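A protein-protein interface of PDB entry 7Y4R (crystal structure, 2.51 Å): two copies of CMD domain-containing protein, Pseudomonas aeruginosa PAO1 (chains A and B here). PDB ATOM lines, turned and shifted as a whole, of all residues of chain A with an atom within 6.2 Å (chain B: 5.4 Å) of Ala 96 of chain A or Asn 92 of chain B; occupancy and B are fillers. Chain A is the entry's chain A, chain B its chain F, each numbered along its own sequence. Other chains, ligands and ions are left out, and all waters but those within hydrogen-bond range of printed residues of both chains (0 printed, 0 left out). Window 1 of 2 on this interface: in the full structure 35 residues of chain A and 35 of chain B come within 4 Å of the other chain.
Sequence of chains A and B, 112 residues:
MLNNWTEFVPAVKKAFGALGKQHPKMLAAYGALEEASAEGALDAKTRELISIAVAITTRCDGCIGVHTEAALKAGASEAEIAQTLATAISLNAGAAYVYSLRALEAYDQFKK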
ATOM      1  N   ARG A  59      -8.491  -0.752 -14.321  1.00  0.00           N
ATOM      2  CA  ARG A  59      -8.592  -0.756 -15.781  1.00  0.00           C
ATOM      3  C   ARG A  59      -7.341  -0.162 -16.427  1.00  0.00           C
ATOM      4  O   ARG A  59      -7.410   0.521 -17.450  1.00  0.00           O
ATOM      5  CB  ARG A  59      -9.855  -0.028 -16.247  1.00  0.00           C
ATOM      6  CG  ARG A  59     -11.112  -0.497 -15.534  1.00  0.00           C
ATOM      7  CD  ARG A  59     -12.373   0.066 -16.166  1.00  0.00           C
ATOM      8  NE  ARG A  59     -13.280   0.625 -15.169  1.00  0.00           N
ATOM      9  CZ  ARG A  59     -13.974  -0.092 -14.295  1.00  0.00           C
ATOM     10  NH1 ARG A  59     -13.902  -1.413 -14.268  1.00  0.00           N
ATOM     11  NH2 ARG A  59     -14.761   0.534 -13.424  1.00  0.00           N
ATOM     12  N   LEU A  91     -16.293  -8.673  -6.622  1.00  0.00           N
ATOM     13  CA  LEU A  91     -16.139  -7.532  -5.727  1.00  0.00           C
ATOM     14  C   LEU A  91     -16.448  -6.214  -6.422  1.00  0.00           C
ATOM     15  O   LEU A  91     -16.922  -5.274  -5.773  1.00  0.00           O
ATOM     16  CB  LEU A  91     -14.724  -7.506  -5.148  1.00  0.00           C
ATOM     17  CG  LEU A  91     -14.620  -8.009  -3.709  1.00  0.00           C
ATOM     18  CD1 LEU A  91     -15.345  -7.066  -2.764  1.00  0.00           C
ATOM     19  CD2 LEU A  91     -15.185  -9.416  -3.600  1.00  0.00           C
ATOM     20  N   ASN A  92     -16.186  -6.123  -7.729  1.00  0.00           N
ATOM     21  CA  ASN A  92     -16.557  -4.922  -8.471  1.00  0.00           C
ATOM     22  C   ASN A  92     -18.068  -4.734  -8.479  1.00  0.00           C
ATOM     23  O   ASN A  92     -18.564  -3.613  -8.306  1.00  0.00           O
ATOM     24  CB  ASN A  92     -16.015  -4.998  -9.898  1.00  0.00           C
ATOM     25  CG  ASN A  92     -14.536  -4.677  -9.977  1.00  0.00           C
ATOM     26  OD1 ASN A  92     -14.145  -3.512 -10.060  1.00  0.00           O
ATOM     27  ND2 ASN A  92     -13.703  -5.712  -9.951  1.00  0.00           N
ATOM     28  N   ALA A  93     -18.817  -5.820  -8.676  1.00  0.00           N
ATOM     29  CA  ALA A  93     -20.269  -5.742  -8.568  1.00  0.00           C
ATOM     30  C   ALA A  93     -20.711  -5.564  -7.121  1.00  0.00           C
ATOM     31  O   ALA A  93     -21.750  -4.948  -6.864  1.00  0.00           O
ATOM     32  CB  ALA A  93     -20.912  -6.990  -9.171  1.00  0.00           C
ATOM     33  N   GLY A  94     -19.935  -6.091  -6.170  1.00  0.00           N
ATOM     34  CA  GLY A  94     -20.296  -5.949  -4.768  1.00  0.00           C
ATOM     35  C   GLY A  94     -20.344  -4.502  -4.320  1.00  0.00           C
ATOM     36  O   GLY A  94     -21.205  -4.115  -3.526  1.00  0.00           O
ATOM     37  N   ALA A  95     -19.418  -3.681  -4.821  1.00  0.00           N
ATOM     38  CA  ALA A  95     -19.463  -2.255  -4.521  1.00  0.00           C
ATOM     39  C   ALA A  95     -20.698  -1.606  -5.134  1.00  0.00           C
ATOM     40  O   ALA A  95     -21.295  -0.703  -4.536  1.00  0.00           O
ATOM     41  CB  ALA A  95     -18.191  -1.571  -5.020  1.00  0.00           C
ATOM     42  N   ALA A  96     -21.097  -2.056  -6.325  1.00  0.00           N
ATOM     43  CA  ALA A  96     -22.312  -1.537  -6.943  1.00  0.00           C
ATOM     44  C   ALA A  96     -23.551  -1.982  -6.177  1.00  0.00           C
ATOM     45  O   ALA A  96     -24.528  -1.231  -6.077  1.00  0.00           O
ATOM     46  CB  ALA A  96     -22.391  -1.980  -8.403  1.00  0.00           C
ATOM     47  N   TYR A  97     -23.530  -3.201  -5.630  1.00  0.00           N
ATOM     48  CA  TYR A  97     -24.655  -3.673  -4.827  1.00  0.00           C
ATOM     49  C   TYR A  97     -24.796  -2.863  -3.545  1.00  0.00           C
ATOM     50  O   TYR A  97     -25.913  -2.507  -3.150  1.00  0.00           O
ATOM     51  CB  TYR A  97     -24.482  -5.156  -4.496  1.00  0.00           C
ATOM     52  CG  TYR A  97     -25.025  -6.105  -5.540  1.00  0.00           C
ATOM     53  CD1 TYR A  97     -26.389  -6.332  -5.659  1.00  0.00           C
ATOM     54  CD2 TYR A  97     -24.171  -6.787  -6.396  1.00  0.00           C
ATOM     55  CE1 TYR A  97     -26.887  -7.205  -6.610  1.00  0.00           C
ATOM     56  CE2 TYR A  97     -24.658  -7.661  -7.348  1.00  0.00           C
ATOM     57  CZ  TYR A  97     -26.017  -7.866  -7.451  1.00  0.00           C
ATOM     58  OH  TYR A  97     -26.505  -8.736  -8.398  1.00  0.00           O
ATOM     59  N   VAL A  98     -23.676  -2.567  -2.882  1.00  0.00           N
ATOM     60  CA  VAL A  98     -23.723  -1.862  -1.604  1.00  0.00           C
ATOM     61  C   VAL A  98     -24.299  -0.463  -1.785  1.00  0.00           C
ATOM     62  O   VAL A  98     -25.150  -0.020  -1.004  1.00  0.00           O
ATOM     63  CB  VAL A  98     -22.321  -1.825  -0.966  1.00  0.00           C
ATOM     64  CG1 VAL A  98     -22.176  -0.623  -0.041  1.00  0.00           C
ATOM     65  CG2 VAL A  98     -22.045  -3.120  -0.217  1.00  0.00           C
ATOM     66  N   TYR A  99     -23.855   0.250  -2.821  1.00  0.00           N
ATOM     67  CA  TYR A  99     -24.357   1.600  -3.049  1.00  0.00           C
ATOM     68  C   TYR A  99     -25.765   1.596  -3.628  1.00  0.00           C
ATOM     69  O   TYR A  99     -26.514   2.557  -3.424  1.00  0.00           O
ATOM     70  CB  TYR A  99     -23.398   2.368  -3.959  1.00  0.00           C
ATOM     71  CG  TYR A  99     -22.238   2.976  -3.204  1.00  0.00           C
ATOM     72  CD1 TYR A  99     -21.100   2.231  -2.923  1.00  0.00           C
ATOM     73  CD2 TYR A  99     -22.286   4.291  -2.760  1.00  0.00           C
ATOM     74  CE1 TYR A  99     -20.040   2.780  -2.228  1.00  0.00           C
ATOM     75  CE2 TYR A  99     -21.230   4.850  -2.065  1.00  0.00           C
ATOM     76  CZ  TYR A  99     -20.109   4.089  -1.801  1.00  0.00           C
ATOM     77  OH  TYR A  99     -19.056   4.641  -1.110  1.00  0.00           O
ATOM     78  N   SER A 100     -26.144   0.535  -4.347  1.00  0.00           N
ATOM     79  CA  SER A 100     -27.536   0.396  -4.761  1.00  0.00           C
ATOM     80  C   SER A 100     -28.447   0.169  -3.563  1.00  0.00           C
ATOM     81  O   SER A 100     -29.603   0.609  -3.572  1.00  0.00           O
ATOM     82  CB  SER A 100     -27.681  -0.749  -5.764  1.00  0.00           C
ATOM     83  OG  SER A 100     -26.887  -0.522  -6.916  1.00  0.00           O
ATOM     84  N   LEU A 101     -27.947  -0.513  -2.528  1.00  0.00           N
ATOM     85  CA  LEU A 101     -28.716  -0.661  -1.297  1.00  0.00           C
ATOM     86  C   LEU A 101     -28.945   0.685  -0.625  1.00  0.00           C
ATOM     87  O   LEU A 101     -29.998   0.905  -0.014  1.00  0.00           O
ATOM     88  CB  LEU A 101     -28.002  -1.619  -0.344  1.00  0.00           C
ATOM     89  CG  LEU A 101     -28.028  -3.101  -0.725  1.00  0.00           C
ATOM     90  CD1 LEU A 101     -26.994  -3.879   0.074  1.00  0.00           C
ATOM     91  CD2 LEU A 101     -29.417  -3.683  -0.523  1.00  0.00           C
ATOM     92  N   ALA B  53     -28.451   5.728 -11.635  1.00  0.00           N
ATOM     93  CA  ALA B  53     -27.517   4.683 -12.045  1.00  0.00           C
ATOM     94  C   ALA B  53     -26.079   5.187 -12.037  1.00  0.00           C
ATOM     95  O   ALA B  53     -25.159   4.457 -11.650  1.00  0.00           O
ATOM     96  CB  ALA B  53     -27.893   4.160 -13.431  1.00  0.00           C
ATOM     97  N   ILE B  56     -24.727   5.708  -8.184  1.00  0.00           N
ATOM     98  CA  ILE B  56     -24.217   4.535  -7.479  1.00  0.00           C
ATOM     99  C   ILE B  56     -22.913   4.061  -8.105  1.00  0.00           C
ATOM    100  O   ILE B  56     -22.078   3.447  -7.428  1.00  0.00           O
ATOM    101  CB  ILE B  56     -25.274   3.415  -7.446  1.00  0.00           C
ATOM    102  CG1 ILE B  56     -25.548   2.878  -8.854  1.00  0.00           C
ATOM    103  CG2 ILE B  56     -26.559   3.913  -6.800  1.00  0.00           C
ATOM    104  CD1 ILE B  56     -24.999   1.485  -9.092  1.00  0.00           C
ATOM    105  N   THR B  57     -22.711   4.331  -9.397  1.00  0.00           N
ATOM    106  CA  THR B  57     -21.434   4.009 -10.026  1.00  0.00           C
ATOM    107  C   THR B  57     -20.353   4.995  -9.603  1.00  0.00           C
ATOM    108  O   THR B  57     -19.223   4.597  -9.299  1.00  0.00           O
ATOM    109  CB  THR B  57     -21.583   3.996 -11.546  1.00  0.00           C
ATOM    110  OG1 THR B  57     -22.640   3.103 -11.919  1.00  0.00           O
ATOM    111  CG2 THR B  57     -20.289   3.546 -12.199  1.00  0.00           C
ATOM    112  N   ARG B  59     -20.455   6.590  -6.879  1.00  0.00           N
ATOM    113  CA  ARG B  59     -20.374   6.449  -5.421  1.00  0.00           C
ATOM    114  C   ARG B  59     -20.496   7.789  -4.701  1.00  0.00           C
ATOM    115  O   ARG B  59     -19.911   7.987  -3.633  1.00  0.00           O
ATOM    116  CB  ARG B  59     -19.085   5.733  -4.999  1.00  0.00           C
ATOM    117  CG  ARG B  59     -18.581   4.691  -5.993  1.00  0.00           C
ATOM    118  CD  ARG B  59     -19.025   3.288  -5.621  1.00  0.00           C
ATOM    119  NE  ARG B  59     -18.209   2.274  -6.278  1.00  0.00           N
ATOM    120  CZ  ARG B  59     -18.674   1.371  -7.130  1.00  0.00           C
ATOM    121  NH1 ARG B  59     -19.958   1.317  -7.447  1.00  0.00           N
ATOM    122  NH2 ARG B  59     -17.832   0.501  -7.679  1.00  0.00           N
ATOM    123  N   THR B  87     -29.716  -2.846 -13.524  1.00  0.00           N
ATOM    124  CA  THR B  87     -29.051  -2.559 -14.790  1.00  0.00           C
ATOM    125  C   THR B  87     -27.714  -1.867 -14.558  1.00  0.00           C
ATOM    126  O   THR B  87     -26.727  -2.163 -15.241  1.00  0.00           O
ATOM    127  CB  THR B  87     -29.953  -1.703 -15.681  1.00  0.00           C
ATOM    128  OG1 THR B  87     -31.244  -2.314 -15.787  1.00  0.00           O
ATOM    129  CG2 THR B  87     -29.350  -1.553 -17.071  1.00  0.00           C
ATOM    130  N   ALA B  88     -27.664  -0.947 -13.592  1.00  0.00           N
ATOM    131  CA  ALA B  88     -26.411  -0.269 -13.279  1.00  0.00           C
ATOM    132  C   ALA B  88     -25.396  -1.235 -12.681  1.00  0.00           C
ATOM    133  O   ALA B  88     -24.194  -1.129 -12.953  1.00  0.00           O
ATOM    134  CB  ALA B  88     -26.670   0.898 -12.326  1.00  0.00           C
ATOM    135  N   ILE B  89     -25.860  -2.181 -11.861  1.00  0.00           N
ATOM    136  CA  ILE B  89     -24.962  -3.179 -11.293  1.00  0.00           C
ATOM    137  C   ILE B  89     -24.406  -4.082 -12.388  1.00  0.00           C
ATOM    138  O   ILE B  89     -23.223  -4.441 -12.375  1.00  0.00           O
ATOM    139  CB  ILE B  89     -25.690  -3.988 -10.203  1.00  0.00           C
ATOM    140  CG1 ILE B  89     -25.859  -3.150  -8.934  1.00  0.00           C
ATOM    141  CG2 ILE B  89     -24.945  -5.278  -9.897  1.00  0.00           C
ATOM    142  CD1 ILE B  89     -26.965  -3.639  -8.026  1.00  0.00           C
ATOM    143  N   SER B  90     -25.247  -4.450 -13.359  1.00  0.00           N
ATOM    144  CA  SER B  90     -24.803  -5.336 -14.431  1.00  0.00           C
ATOM    145  C   SER B  90     -23.711  -4.689 -15.273  1.00  0.00           C
ATOM    146  O   SER B  90     -22.747  -5.355 -15.670  1.00  0.00           O
ATOM    147  CB  SER B  90     -25.992  -5.732 -15.307  1.00  0.00           C
ATOM    148  OG  SER B  90     -25.578  -6.557 -16.382  1.00  0.00           O
ATOM    149  N   LEU B  91     -23.842  -3.392 -15.556  1.00  0.00           N
ATOM    150  CA  LEU B  91     -22.827  -2.711 -16.353  1.00  0.00           C
ATOM    151  C   LEU B  91     -21.537  -2.509 -15.568  1.00  0.00           C
ATOM    152  O   LEU B  91     -20.451  -2.507 -16.158  1.00  0.00           O
ATOM    153  CB  LEU B  91     -23.364  -1.371 -16.854  1.00  0.00           C
ATOM    154  CG  LEU B  91     -23.735  -1.330 -18.336  1.00  0.00           C
ATOM    155  CD1 LEU B  91     -22.487  -1.367 -19.201  1.00  0.00           C
ATOM    156  CD2 LEU B  91     -24.657  -2.490 -18.675  1.00  0.00           C
ATOM    157  N   ASN B  92     -21.635  -2.338 -14.248  1.00  0.00           N
ATOM    158  CA  ASN B  92     -20.435  -2.250 -13.422  1.00  0.00           C
ATOM    159  C   ASN B  92     -19.647  -3.552 -13.473  1.00  0.00           C
ATOM    160  O   ASN B  92     -18.428  -3.549 -13.682  1.00  0.00           O
ATOM    161  CB  ASN B  92     -20.812  -1.904 -11.981  1.00  0.00           C
ATOM    162  CG  ASN B  92     -21.047  -0.422 -11.780  1.00  0.00           C
ATOM    163  OD1 ASN B  92     -20.172   0.296 -11.294  1.00  0.00           O
ATOM    164  ND2 ASN B  92     -22.233   0.047 -12.149  1.00  0.00           N
ATOM    165  N   ALA B  93     -20.332  -4.683 -13.281  1.00  0.00           N
ATOM    166  CA  ALA B  93     -19.677  -5.977 -13.426  1.00  0.00           C
ATOM    167  C   ALA B  93     -19.224  -6.210 -14.861  1.00  0.00           C
ATOM    168  O   ALA B  93     -18.203  -6.868 -15.091  1.00  0.00           O
ATOM    169  CB  ALA B  93     -20.614  -7.098 -12.978  1.00  0.00           C
ATOM    170  N   GLY B  94     -19.965  -5.676 -15.835  1.00  0.00           N
ATOM    171  CA  GLY B  94     -19.559  -5.822 -17.223  1.00  0.00           C
ATOM    172  C   GLY B  94     -18.216  -5.181 -17.510  1.00  0.00           C
ATOM    173  O   GLY B  94     -17.395  -5.740 -18.239  1.00  0.00           O
ATOM    174  N   ALA B  95     -17.970  -4.001 -16.933  1.00  0.00           N
ATOM    175  CA  ALA B  95     -16.687  -3.333 -17.129  1.00  0.00           C
ATOM    176  C   ALA B  95     -15.539  -4.176 -16.589  1.00  0.00           C
ATOM    177  O   ALA B  95     -14.457  -4.223 -17.187  1.00  0.00           O
ATOM    178  CB  ALA B  95     -16.703  -1.955 -16.465  1.00  0.00           C
ATOM    179  N   ALA B  96     -15.756  -4.852 -15.458  1.00  0.00           N
ATOM    180  CA  ALA B  96     -14.741  -5.761 -14.942  1.00  0.00           C
ATOM    181  C   ALA B  96     -14.594  -6.991 -15.827  1.00  0.00           C
ATOM    182  O   ALA B  96     -13.487  -7.520 -15.971  1.00  0.00           O
ATOM    183  CB  ALA B  96     -15.080  -6.171 -13.507  1.00  0.00           C
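The backbone carbonyl oxygen of Ile 56 of chain B sits at hydrogen-bond distance from the guanidinium group of Arg 59 of chain B, 3.0 Å away.
OG of Ser 100 of chain A is in hydrogen-bond range of O of Ala 96 of chain A.
The side-chain amide nitrogen of Asn 92 of chain B lies within hydrogen-bond range of the backbone carbonyl oxygen of Ala 88 of chain B (2.4 Å).
The side-chain amide nitrogen (ND2) of Asn 92 of chain B is in hydrogen-bond range of the side-chain hydroxyl (OG1) of Thr 57 of chain B (3.1 Å).
Among the printed residues, pairs that only touch across the chains: Ser 100 of chain A with Ile 89 of chain B (3.3 Å), Ala 95 of chain A with Arg 59 of chain B (3.4 Å), Tyr 97 of chain A with Ile 89 of chain B (3.5 Å), Ser 100 of chain A with Ile 56 of chain B (3.5 Å), Tyr 99 of chain A with Arg 59 of chain B (3.6 Å), Arg 59 of chain A with Ala 95 of chain B (3.6 Å), Tyr 99 of chain A with Ile 56 of chain B (3.6 Å), Ala 96 of chain A with Ile 89 of chain B (3.7 Å), Ala 96 of chain A with Arg 59 of chain B (3.7 Å), Ala 93 of chain A with Ala 93 of chain B (3.8 Å), Asn 92 of chain A with Ala 96 of chain B (3.8 Å) and Ala 96 of chain A with Asn 92 of chain B (3.9 Å).
Of chain B, only Arg 59 (3.7 Å), Ile 89 (3.7 Å) and Asn 92 (3.9 Å) come within 4 Å of Ala 96 of chain A.
Asn 92 of chain B touches just one residue of chain A: Ala 96.
Of the printed residues of chain A, Ala 93 of chain B touches Ala 93.
Printed residues of chain A within 4 Å of Ala 95 of chain B: Arg 59.
Printed residues of chain A within 4 Å of Ile 56 of chain B: Tyr 99 (3.6 Å) and Ser 100 (3.5 Å).
Printed residues of chain B within 4 Å of Ala 95 of chain A: Arg 59 (3.4 Å).
Printed residues of chain A within 4 Å of Arg 59 of chain B: Ala 95, Ala 96 and Tyr 99.
The nearest printed residue of chain B that does not touch Arg 59 of chain A is Ala 96 of chain B (4.1 Å).
Of the 14 printed residues of chain B, 7 touch a printed residue of chain A.
Hydrophobic or aromatic side chains of chain B that line the printed part of chain A: Ile 56, Ile 89, Ala 93, Ala 95 and Ala 96.
Of the 12 printed residues of chain A, 8 touch a printed residue of chain B.
Printed residues of chain A that touch a printed residue of chain B: Arg 59, Asn 92, Ala 93, Ala 95, Ala 96, Tyr 97, Tyr 99 and Ser 100.
Among the printed residues, 12 pairs touch across the chains.
Among the printed residues, no Asp or Glu carboxylate lies within 4 Å of a Lys or Arg side-chain nitrogen of the other chain.
Arg 59 of chain A touches Ala 95 of chain B, and with the chains exchanged Ala 95 of chain A touches Arg 59 of chain B.
Asn 92 of chain A touches Ala 96 of chain B, and with the chains exchanged Ala 96 of chain A touches Asn 92 of chain B.
Ala 93 of chain B touches its own counterpart, Ala 93 of chain A.
Ala 96 of chain A touches Arg 59 of chain B, but with the chains exchanged Arg 59 of chain A does not touch Ala 96 of chain B (4.1 Å).
Positions printed for both chains: 59, 91, 92, 93, 94, 95 and 96.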
